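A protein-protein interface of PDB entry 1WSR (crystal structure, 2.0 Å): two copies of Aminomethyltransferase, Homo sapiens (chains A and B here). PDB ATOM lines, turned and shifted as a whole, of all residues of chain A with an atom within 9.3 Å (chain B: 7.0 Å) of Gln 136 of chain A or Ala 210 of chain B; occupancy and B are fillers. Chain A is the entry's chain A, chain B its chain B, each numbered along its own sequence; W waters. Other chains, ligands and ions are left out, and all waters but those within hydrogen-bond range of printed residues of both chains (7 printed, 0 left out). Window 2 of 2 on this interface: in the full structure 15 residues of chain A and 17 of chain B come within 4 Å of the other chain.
Gln 136 of chain A touches three residues of chain B.
Ala 210 of chain B touches one residue of chain A.
Val 209 of chain B touches three residues of chain A.
No residue of chain A comes within 4 Å of Gly 211 of chain B.
Printed residues of chain B within 4 Å of Asn 137 of chain A: Val 209 (3.7 Å).
Of the printed residues of chain B, Arg 133 of chain A touches Pro 9 and Val 209.
Of the printed residues of chain A, Asp 148 of chain B touches Gln 136 (3.2 Å).
Met 128 of chain A touches none of the printed residues of chain B.
CD of Arg 133 of chain A touches CD of Pro 9 of chain B, 3.9 Å away.
Arg 133 of chain A touches Val 209 of chain B (O to CG1, 3.5 Å).
Gln 136 of chain A touches Val 209 of chain B.
O of Gln 136 of chain A touches CB of Ala 210 of chain B, at 3.6 Å.
Asn 137 of chain A touches Val 209 of chain B (N to CG1, 3.7 Å).
No position is printed for both chains.
Of the 6 pairs that touch across the chains among the printed residues, none has its exchanged pair printed and touching as well.
Printed residues of chain B that touch a printed residue of chain A: Pro 9, Asp 148, Val 209 and Ala 210.
Hydrophobic or aromatic side chains of chain B that line the printed part of chain A: Pro 9, Val 209 and Ala 210.
The side-chain carboxylate of Asp 130 of chain A lies within salt-bridge range of the guanidinium group of Arg 133 of chain A (2.9 Å).
The side-chain amide nitrogen (NE2) of Gln 136 of chain A lies within hydrogen-bond range of the backbone carbonyl oxygen (O) of Val 142 of chain A (2.8 Å).
The side-chain amide nitrogen (NE2) of Gln 136 of chain A sits at hydrogen-bond distance from the side-chain carboxylate (OD2) of Asp 148 of chain B.
Water W1 bridges the side-chain carboxylate (OD2) of Asp 148 of chain B and the backbone NH (N) of Leu 144 of chain A.
Water W3 lies within hydrogen-bond range of the backbone carbonyl oxygen (O) of Val 209 of chain B (2.6 Å), the side-chain amide oxygen (OD1) of Asn 137 of chain A (2.9 Å), the backbone NH (N) of Val 213 of chain B (3.0 Å) and the backbone NH (N) of Ala 212 of chain B (3.3 Å).
Water W6 bridges O of Asp 148 of chain B and OE1 of Gln 136 of chain A.
Water W5 lies within hydrogen-bond range of the guanidinium group of Arg 133 of chain A and the backbone carbonyl oxygen of Asp 148 of chain B.
Water W7 lies within hydrogen-bond range of OE1 of Gln 136 of chain A (2.9 Å), N of Val 209 of chain B (2.9 Å) and OD1 of Asp 148 of chain B (2.9 Å).
Water W4 bridges the backbone carbonyl oxygen of Leu 144 of chain A (3.4 Å) and the side-chain carboxylate of Asp 148 of chain B (3.5 Å).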
ATOM      1  N   LEU A  62      -9.584 -10.061 -25.953  1.00  0.00           N
ATOM      2  CA  LEU A  62     -10.603  -9.961 -26.990  1.00  0.00           C
ATOM      3  C   LEU A  62     -11.988 -10.290 -26.449  1.00  0.00           C
ATOM      4  O   LEU A  62     -12.127 -10.743 -25.315  1.00  0.00           O
ATOM      5  CB  LEU A  62     -10.282 -10.922 -28.139  1.00  0.00           C
ATOM      6  CG  LEU A  62      -8.910 -10.834 -28.816  1.00  0.00           C
ATOM      7  CD1 LEU A  62      -7.853 -11.486 -27.940  1.00  0.00           C
ATOM      8  CD2 LEU A  62      -8.972 -11.546 -30.157  1.00  0.00           C
ATOM      9  N   GLY A  63     -13.008 -10.063 -27.272  1.00  0.00           N
ATOM     10  CA  GLY A  63     -14.367 -10.364 -26.861  1.00  0.00           C
ATOM     11  C   GLY A  63     -15.167  -9.159 -26.412  1.00  0.00           C
ATOM     12  O   GLY A  63     -14.603  -8.126 -26.053  1.00  0.00           O
ATOM     13  N   ASP A  65     -16.844  -8.931 -23.752  1.00  0.00           N
ATOM     14  CA  ASP A  65     -16.739  -8.765 -22.306  1.00  0.00           C
ATOM     15  C   ASP A  65     -15.310  -8.498 -21.840  1.00  0.00           C
ATOM     16  O   ASP A  65     -14.974  -8.739 -20.680  1.00  0.00           O
ATOM     17  CB  ASP A  65     -17.287 -10.001 -21.589  1.00  0.00           C
ATOM     18  CG  ASP A  65     -18.770 -10.197 -21.824  1.00  0.00           C
ATOM     19  OD1 ASP A  65     -19.156 -10.565 -22.954  1.00  0.00           O
ATOM     20  OD2 ASP A  65     -19.550  -9.971 -20.879  1.00  0.00           O
ATOM     21  N   LEU A  69     -13.908  -8.118 -17.921  1.00  0.00           N
ATOM     22  CA  LEU A  69     -12.851  -8.976 -17.403  1.00  0.00           C
ATOM     23  C   LEU A  69     -11.728  -8.142 -16.802  1.00  0.00           C
ATOM     24  O   LEU A  69     -11.308  -8.373 -15.667  1.00  0.00           O
ATOM     25  CB  LEU A  69     -12.290  -9.872 -18.516  1.00  0.00           C
ATOM     26  CG  LEU A  69     -11.110 -10.784 -18.144  1.00  0.00           C
ATOM     27  CD1 LEU A  69     -11.119 -12.019 -19.025  1.00  0.00           C
ATOM     28  CD2 LEU A  69      -9.793 -10.036 -18.286  1.00  0.00           C
ATOM     29  N   MET A 128      -5.027 -13.877 -15.578  1.00  0.00           N
ATOM     30  CA  MET A 128      -5.925 -13.489 -16.654  1.00  0.00           C
ATOM     31  C   MET A 128      -6.602 -14.711 -17.266  1.00  0.00           C
ATOM     32  O   MET A 128      -7.789 -14.664 -17.591  1.00  0.00           O
ATOM     33  CB  MET A 128      -5.165 -12.685 -17.713  1.00  0.00           C
ATOM     34  CG  MET A 128      -4.689 -11.332 -17.184  1.00  0.00           C
ATOM     35  SD  MET A 128      -3.989 -10.246 -18.443  1.00  0.00           S
ATOM     36  CE  MET A 128      -2.311 -10.904 -18.561  1.00  0.00           C
ATOM     37  N   GLN A 129      -5.855 -15.805 -17.410  1.00  0.00           N
ATOM     38  CA  GLN A 129      -6.414 -17.039 -17.958  1.00  0.00           C
ATOM     39  C   GLN A 129      -7.537 -17.548 -17.059  1.00  0.00           C
ATOM     40  O   GLN A 129      -8.591 -17.964 -17.543  1.00  0.00           O
ATOM     41  CB  GLN A 129      -5.348 -18.131 -18.050  1.00  0.00           C
ATOM     42  CG  GLN A 129      -4.242 -17.885 -19.053  1.00  0.00           C
ATOM     43  CD  GLN A 129      -3.269 -19.053 -19.105  1.00  0.00           C
ATOM     44  OE1 GLN A 129      -2.840 -19.558 -18.066  1.00  0.00           O
ATOM     45  NE2 GLN A 129      -2.915 -19.483 -20.311  1.00  0.00           N
ATOM     46  N   ASP A 130      -7.303 -17.528 -15.749  1.00  0.00           N
ATOM     47  CA  ASP A 130      -8.308 -17.990 -14.799  1.00  0.00           C
ATOM     48  C   ASP A 130      -9.599 -17.183 -14.929  1.00  0.00           C
ATOM     49  O   ASP A 130     -10.695 -17.744 -14.867  1.00  0.00           O
ATOM     50  CB  ASP A 130      -7.798 -17.881 -13.356  1.00  0.00           C
ATOM     51  CG  ASP A 130      -6.677 -18.865 -13.043  1.00  0.00           C
ATOM     52  OD1 ASP A 130      -6.480 -19.827 -13.815  1.00  0.00           O
ATOM     53  OD2 ASP A 130      -5.999 -18.677 -12.010  1.00  0.00           O
ATOM     54  N   LYS A 131      -9.475 -15.871 -15.110  1.00  0.00           N
ATOM     55  CA  LYS A 131     -10.659 -15.021 -15.232  1.00  0.00           C
ATOM     56  C   LYS A 131     -11.379 -15.284 -16.551  1.00  0.00           C
ATOM     57  O   LYS A 131     -12.611 -15.316 -16.605  1.00  0.00           O
ATOM     58  CB  LYS A 131     -10.281 -13.543 -15.127  1.00  0.00           C
ATOM     59  CG  LYS A 131     -11.414 -12.684 -14.583  1.00  0.00           C
ATOM     60  CD  LYS A 131     -11.770 -13.147 -13.171  1.00  0.00           C
ATOM     61  CE  LYS A 131     -12.922 -12.371 -12.577  1.00  0.00           C
ATOM     62  NZ  LYS A 131     -13.269 -12.902 -11.231  1.00  0.00           N
ATOM     63  N   VAL A 132     -10.607 -15.465 -17.617  1.00  0.00           N
ATOM     64  CA  VAL A 132     -11.182 -15.772 -18.922  1.00  0.00           C
ATOM     65  C   VAL A 132     -11.997 -17.062 -18.790  1.00  0.00           C
ATOM     66  O   VAL A 132     -13.152 -17.124 -19.208  1.00  0.00           O
ATOM     67  CB  VAL A 132     -10.076 -15.985 -19.989  1.00  0.00           C
ATOM     68  CG1 VAL A 132     -10.658 -16.667 -21.224  1.00  0.00           C
ATOM     69  CG2 VAL A 132      -9.461 -14.648 -20.376  1.00  0.00           C
ATOM     70  N   ARG A 133     -11.384 -18.083 -18.195  1.00  0.00           N
ATOM     71  CA  ARG A 133     -12.030 -19.381 -18.002  1.00  0.00           C
ATOM     72  C   ARG A 133     -13.331 -19.228 -17.216  1.00  0.00           C
ATOM     73  O   ARG A 133     -14.358 -19.821 -17.558  1.00  0.00           O
ATOM     74  CB  ARG A 133     -11.086 -20.323 -17.243  1.00  0.00           C
ATOM     75  CG  ARG A 133     -11.557 -21.779 -17.158  1.00  0.00           C
ATOM     76  CD  ARG A 133     -10.593 -22.624 -16.322  1.00  0.00           C
ATOM     77  NE  ARG A 133      -9.206 -22.348 -16.688  1.00  0.00           N
ATOM     78  CZ  ARG A 133      -8.302 -21.829 -15.861  1.00  0.00           C
ATOM     79  NH1 ARG A 133      -8.630 -21.539 -14.608  1.00  0.00           N
ATOM     80  NH2 ARG A 133      -7.080 -21.563 -16.298  1.00  0.00           N
ATOM     81  N   GLU A 134     -13.272 -18.427 -16.159  1.00  0.00           N
ATOM     82  CA  GLU A 134     -14.422 -18.183 -15.300  1.00  0.00           C
ATOM     83  C   GLU A 134     -15.578 -17.572 -16.086  1.00  0.00           C
ATOM     84  O   GLU A 134     -16.714 -18.035 -15.990  1.00  0.00           O
ATOM     85  CB  GLU A 134     -14.021 -17.248 -14.155  1.00  0.00           C
ATOM     86  CG  GLU A 134     -15.077 -17.063 -13.082  1.00  0.00           C
ATOM     87  CD  GLU A 134     -14.674 -16.020 -12.051  1.00  0.00           C
ATOM     88  OE1 GLU A 134     -13.558 -16.126 -11.500  1.00  0.00           O
ATOM     89  OE2 GLU A 134     -15.474 -15.095 -11.794  1.00  0.00           O
ATOM     90  N   LEU A 135     -15.282 -16.537 -16.869  1.00  0.00           N
ATOM     91  CA  LEU A 135     -16.300 -15.854 -17.661  1.00  0.00           C
ATOM     92  C   LEU A 135     -16.849 -16.701 -18.807  1.00  0.00           C
ATOM     93  O   LEU A 135     -18.041 -16.640 -19.113  1.00  0.00           O
ATOM     94  CB  LEU A 135     -15.747 -14.536 -18.215  1.00  0.00           C
ATOM     95  CG  LEU A 135     -15.257 -13.535 -17.166  1.00  0.00           C
ATOM     96  CD1 LEU A 135     -14.895 -12.220 -17.835  1.00  0.00           C
ATOM     97  CD2 LEU A 135     -16.340 -13.315 -16.123  1.00  0.00           C
ATOM     98  N   GLN A 136     -15.988 -17.483 -19.447  1.00  0.00           N
ATOM     99  CA  GLN A 136     -16.436 -18.330 -20.544  1.00  0.00           C
ATOM    100  C   GLN A 136     -17.395 -19.396 -20.016  1.00  0.00           C
ATOM    101  O   GLN A 136     -18.339 -19.788 -20.701  1.00  0.00           O
ATOM    102  CB  GLN A 136     -15.247 -19.002 -21.234  1.00  0.00           C
ATOM    103  CG  GLN A 136     -14.262 -18.035 -21.888  1.00  0.00           C
ATOM    104  CD  GLN A 136     -13.198 -18.756 -22.691  1.00  0.00           C
ATOM    105  OE1 GLN A 136     -12.821 -19.882 -22.365  1.00  0.00           O
ATOM    106  NE2 GLN A 136     -12.696 -18.107 -23.736  1.00  0.00           N
ATOM    107  N   ASN A 137     -17.151 -19.862 -18.796  1.00  0.00           N
ATOM    108  CA  ASN A 137     -18.002 -20.878 -18.189  1.00  0.00           C
ATOM    109  C   ASN A 137     -19.371 -20.298 -17.851  1.00  0.00           C
ATOM    110  O   ASN A 137     -20.336 -21.036 -17.642  1.00  0.00           O
ATOM    111  CB  ASN A 137     -17.357 -21.428 -16.918  1.00  0.00           C
ATOM    112  CG  ASN A 137     -18.171 -22.539 -16.287  1.00  0.00           C
ATOM    113  OD1 ASN A 137     -18.392 -23.588 -16.898  1.00  0.00           O
ATOM    114  ND2 ASN A 137     -18.629 -22.317 -15.058  1.00  0.00           N
ATOM    115  N   GLN A 138     -19.448 -18.973 -17.794  1.00  0.00           N
ATOM    116  CA  GLN A 138     -20.700 -18.294 -17.491  1.00  0.00           C
ATOM    117  C   GLN A 138     -21.381 -17.887 -18.796  1.00  0.00           C
ATOM    118  O   GLN A 138     -22.372 -17.157 -18.790  1.00  0.00           O
ATOM    119  CB  GLN A 138     -20.436 -17.060 -16.621  1.00  0.00           C
ATOM    120  CG  GLN A 138     -19.704 -17.378 -15.320  1.00  0.00           C
ATOM    121  CD  GLN A 138     -19.409 -16.143 -14.485  1.00  0.00           C
ATOM    122  OE1 GLN A 138     -18.851 -15.164 -14.978  1.00  0.00           O
ATOM    123  NE2 GLN A 138     -19.773 -16.192 -13.208  1.00  0.00           N
ATOM    124  N   GLY A 139     -20.832 -18.365 -19.910  1.00  0.00           N
ATOM    125  CA  GLY A 139     -21.395 -18.063 -21.215  1.00  0.00           C
ATOM    126  C   GLY A 139     -20.995 -16.734 -21.834  1.00  0.00           C
ATOM    127  O   GLY A 139     -21.493 -16.378 -22.902  1.00  0.00           O
ATOM    128  N   ARG A 140     -20.097 -16.002 -21.183  1.00  0.00           N
ATOM    129  CA  ARG A 140     -19.652 -14.705 -21.689  1.00  0.00           C
ATOM    130  C   ARG A 140     -18.659 -14.830 -22.845  1.00  0.00           C
ATOM    131  O   ARG A 140     -18.049 -15.881 -23.046  1.00  0.00           O
ATOM    132  CB  ARG A 140     -19.012 -13.889 -20.562  1.00  0.00           C
ATOM    133  CG  ARG A 140     -19.966 -13.476 -19.452  1.00  0.00           C
ATOM    134  CD  ARG A 140     -20.989 -12.465 -19.944  1.00  0.00           C
ATOM    135  NE  ARG A 140     -21.825 -11.954 -18.860  1.00  0.00           N
ATOM    136  CZ  ARG A 140     -21.370 -11.244 -17.831  1.00  0.00           C
ATOM    137  NH1 ARG A 140     -20.079 -10.955 -17.738  1.00  0.00           N
ATOM    138  NH2 ARG A 140     -22.208 -10.819 -16.893  1.00  0.00           N
ATOM    139  N   ASP A 141     -18.498 -13.740 -23.591  1.00  0.00           N
ATOM    140  CA  ASP A 141     -17.589 -13.697 -24.730  1.00  0.00           C
ATOM    141  C   ASP A 141     -16.289 -12.971 -24.406  1.00  0.00           C
ATOM    142  O   ASP A 141     -16.256 -11.743 -24.342  1.00  0.00           O
ATOM    143  CB  ASP A 141     -18.251 -12.987 -25.909  1.00  0.00           C
ATOM    144  CG  ASP A 141     -17.311 -12.821 -27.088  1.00  0.00           C
ATOM    145  OD1 ASP A 141     -17.464 -11.841 -27.846  1.00  0.00           O
ATOM    146  OD2 ASP A 141     -16.420 -13.675 -27.262  1.00  0.00           O
ATOM    147  N   VAL A 142     -15.215 -13.728 -24.212  1.00  0.00           N
ATOM    148  CA  VAL A 142     -13.923 -13.127 -23.913  1.00  0.00           C
ATOM    149  C   VAL A 142     -12.808 -14.117 -24.224  1.00  0.00           C
ATOM    150  O   VAL A 142     -13.017 -15.333 -24.204  1.00  0.00           O
ATOM    151  CB  VAL A 142     -13.840 -12.686 -22.427  1.00  0.00           C
ATOM    152  CG1 VAL A 142     -13.764 -13.904 -21.518  1.00  0.00           C
ATOM    153  CG2 VAL A 142     -12.643 -11.775 -22.219  1.00  0.00           C
ATOM    154  N   GLY A 143     -11.631 -13.589 -24.533  1.00  0.00           N
ATOM    155  CA  GLY A 143     -10.492 -14.432 -24.842  1.00  0.00           C
ATOM    156  C   GLY A 143      -9.204 -13.661 -24.652  1.00  0.00           C
ATOM    157  O   GLY A 143      -9.219 -12.436 -24.506  1.00  0.00           O
ATOM    158  N   LEU A 144      -8.083 -14.373 -24.655  1.00  0.00           N
ATOM    159  CA  LEU A 144      -6.790 -13.743 -24.479  1.00  0.00           C
ATOM    160  C   LEU A 144      -5.756 -14.306 -25.447  1.00  0.00           C
ATOM    161  O   LEU A 144      -5.787 -15.487 -25.785  1.00  0.00           O
ATOM    162  CB  LEU A 144      -6.319 -13.933 -23.032  1.00  0.00           C
ATOM    163  CG  LEU A 144      -4.863 -13.605 -22.687  1.00  0.00           C
ATOM    164  CD1 LEU A 144      -4.756 -13.246 -21.213  1.00  0.00           C
ATOM    165  CD2 LEU A 144      -3.969 -14.797 -23.017  1.00  0.00           C
ATOM    166  N   PRO B   9     -12.767 -26.026 -15.386  1.00  0.00           N
ATOM    167  CA  PRO B   9     -14.201 -25.753 -15.531  1.00  0.00           C
ATOM    168  C   PRO B   9     -15.087 -26.757 -14.787  1.00  0.00           C
ATOM    169  O   PRO B   9     -16.265 -26.492 -14.548  1.00  0.00           O
ATOM    170  CB  PRO B   9     -14.415 -25.812 -17.044  1.00  0.00           C
ATOM    171  CG  PRO B   9     -13.083 -25.382 -17.590  1.00  0.00           C
ATOM    172  CD  PRO B   9     -12.119 -26.138 -16.704  1.00  0.00           C
ATOM    173  N   ASP B 148      -7.502 -22.230 -24.810  1.00  0.00           N
ATOM    174  CA  ASP B 148      -8.164 -22.053 -23.526  1.00  0.00           C
ATOM    175  C   ASP B 148      -9.187 -23.146 -23.219  1.00  0.00           C
ATOM    176  O   ASP B 148      -9.920 -23.051 -22.237  1.00  0.00           O
ATOM    177  CB  ASP B 148      -8.836 -20.674 -23.454  1.00  0.00           C
ATOM    178  CG  ASP B 148      -9.754 -20.402 -24.635  1.00  0.00           C
ATOM    179  OD1 ASP B 148     -10.279 -21.372 -25.222  1.00  0.00           O
ATOM    180  OD2 ASP B 148      -9.964 -19.211 -24.965  1.00  0.00           O
ATOM    181  N   ASN B 149      -9.219 -24.186 -24.048  1.00  0.00           N
ATOM    182  CA  ASN B 149     -10.151 -25.303 -23.872  1.00  0.00           C
ATOM    183  C   ASN B 149      -9.897 -26.149 -22.631  1.00  0.00           C
ATOM    184  O   ASN B 149      -8.799 -26.156 -22.076  1.00  0.00           O
ATOM    185  CB  ASN B 149     -10.093 -26.251 -25.078  1.00  0.00           C
ATOM    186  CG  ASN B 149     -10.784 -25.694 -26.304  1.00  0.00           C
ATOM    187  OD1 ASN B 149     -11.366 -24.615 -26.268  1.00  0.00           O
ATOM    188  ND2 ASN B 149     -10.726 -26.443 -27.404  1.00  0.00           N
ATOM    189  N   VAL B 187     -21.879 -30.356 -28.297  1.00  0.00           N
ATOM    190  CA  VAL B 187     -20.857 -29.319 -28.211  1.00  0.00           C
ATOM    191  C   VAL B 187     -19.993 -29.346 -29.468  1.00  0.00           C
ATOM    192  O   VAL B 187     -19.234 -30.289 -29.687  1.00  0.00           O
ATOM    193  CB  VAL B 187     -19.947 -29.527 -26.979  1.00  0.00           C
ATOM    194  CG1 VAL B 187     -18.972 -28.365 -26.849  1.00  0.00           C
ATOM    195  CG2 VAL B 187     -20.792 -29.653 -25.726  1.00  0.00           C
ATOM    196  N   VAL B 207     -12.329 -29.640 -25.323  1.00  0.00           N
ATOM    197  CA  VAL B 207     -13.633 -29.006 -25.440  1.00  0.00           C
ATOM    198  C   VAL B 207     -13.671 -27.560 -24.955  1.00  0.00           C
ATOM    199  O   VAL B 207     -13.070 -27.218 -23.938  1.00  0.00           O
ATOM    200  CB  VAL B 207     -14.681 -29.839 -24.651  1.00  0.00           C
ATOM    201  CG1 VAL B 207     -14.174 -30.089 -23.231  1.00  0.00           C
ATOM    202  CG2 VAL B 207     -16.025 -29.130 -24.617  1.00  0.00           C
ATOM    203  N   PRO B 208     -14.375 -26.685 -25.691  1.00  0.00           N
ATOM    204  CA  PRO B 208     -14.465 -25.280 -25.285  1.00  0.00           C
ATOM    205  C   PRO B 208     -15.015 -25.208 -23.864  1.00  0.00           C
ATOM    206  O   PRO B 208     -15.917 -25.967 -23.503  1.00  0.00           O
ATOM    207  CB  PRO B 208     -15.426 -24.689 -26.311  1.00  0.00           C
ATOM    208  CG  PRO B 208     -15.108 -25.491 -27.548  1.00  0.00           C
ATOM    209  CD  PRO B 208     -15.028 -26.899 -26.995  1.00  0.00           C
ATOM    210  N   VAL B 209     -14.467 -24.301 -23.066  1.00  0.00           N
ATOM    211  CA  VAL B 209     -14.888 -24.135 -21.682  1.00  0.00           C
ATOM    212  C   VAL B 209     -16.405 -24.052 -21.504  1.00  0.00           C
ATOM    213  O   VAL B 209     -16.962 -24.704 -20.623  1.00  0.00           O
ATOM    214  CB  VAL B 209     -14.232 -22.877 -21.064  1.00  0.00           C
ATOM    215  CG1 VAL B 209     -14.824 -22.587 -19.690  1.00  0.00           C
ATOM    216  CG2 VAL B 209     -12.726 -23.093 -20.951  1.00  0.00           C
ATOM    217  N   ALA B 210     -17.067 -23.269 -22.350  1.00  0.00           N
ATOM    218  CA  ALA B 210     -18.515 -23.084 -22.266  1.00  0.00           C
ATOM    219  C   ALA B 210     -19.330 -24.375 -22.342  1.00  0.00           C
ATOM    220  O   ALA B 210     -20.460 -24.429 -21.850  1.00  0.00           O
ATOM    221  CB  ALA B 210     -18.978 -22.108 -23.358  1.00  0.00           C
ATOM    222  N   GLY B 211     -18.769 -25.415 -22.953  1.00  0.00           N
ATOM    223  CA  GLY B 211     -19.496 -26.667 -23.059  1.00  0.00           C
ATOM    224  C   GLY B 211     -18.885 -27.823 -22.285  1.00  0.00           C
ATOM    225  O   GLY B 211     -19.359 -28.958 -22.391  1.00  0.00           O
ATOM    226  N   ALA B 212     -17.851 -27.540 -21.497  1.00  0.00           N
ATOM    227  CA  ALA B 212     -17.163 -28.572 -20.719  1.00  0.00           C
ATOM    228  C   ALA B 212     -18.047 -29.314 -19.720  1.00  0.00           C
ATOM    229  O   ALA B 212     -18.050 -30.547 -19.682  1.00  0.00           O
ATOM    230  CB  ALA B 212     -15.963 -27.962 -19.991  1.00  0.00           C
ATOM    231  N   VAL B 213     -18.787 -28.576 -18.900  1.00  0.00           N
ATOM    232  CA  VAL B 213     -19.653 -29.213 -17.913  1.00  0.00           C
ATOM    233  C   VAL B 213     -20.746 -30.029 -18.595  1.00  0.00           C
ATOM    234  O   VAL B 213     -21.060 -31.139 -18.166  1.00  0.00           O
ATOM    235  CB  VAL B 213     -20.291 -28.169 -16.975  1.00  0.00           C
ATOM    236  CG1 VAL B 213     -21.294 -28.838 -16.049  1.00  0.00           C
ATOM    237  CG2 VAL B 213     -19.204 -27.490 -16.160  1.00  0.00           C
ATOM    238  N   HIS B 214     -21.321 -29.479 -19.662  1.00  0.00           N
ATOM    239  CA  HIS B 214     -22.367 -30.179 -20.402  1.00  0.00           C
ATOM    240  C   HIS B 214     -21.845 -31.516 -20.927  1.00  0.00           C
ATOM    241  O   HIS B 214     -22.515 -32.544 -20.820  1.00  0.00           O
ATOM    242  CB  HIS B 214     -22.844 -29.333 -21.585  1.00  0.00           C
ATOM    243  CG  HIS B 214     -23.845 -30.030 -22.455  1.00  0.00           C
ATOM    244  ND1 HIS B 214     -25.156 -30.220 -22.076  1.00  0.00           N
ATOM    245  CD2 HIS B 214     -23.718 -30.607 -23.673  1.00  0.00           C
ATOM    246  CE1 HIS B 214     -25.795 -30.884 -23.023  1.00  0.00           C
ATOM    247  NE2 HIS B 214     -24.944 -31.131 -24.004  1.00  0.00           N
HETATM  248  O   HOH W   1      -8.254 -17.387 -24.162  1.00  0.00           O
HETATM  249  O   HOH W   2     -21.554 -22.722 -20.182  1.00  0.00           O
HETATM  250  O   HOH W   3     -18.803 -25.616 -18.973  1.00  0.00           O
HETATM  251  O   HOH W   4      -6.755 -18.697 -26.141  1.00  0.00           O
HETATM  252  O   HOH W   5      -8.909 -22.839 -19.383  1.00  0.00           O
HETATM  253  O   HOH W   6     -10.581 -20.769 -20.844  1.00  0.00           O
HETATM  254  O   HOH W   7     -12.925 -22.104 -24.197  1.00  0.00           O
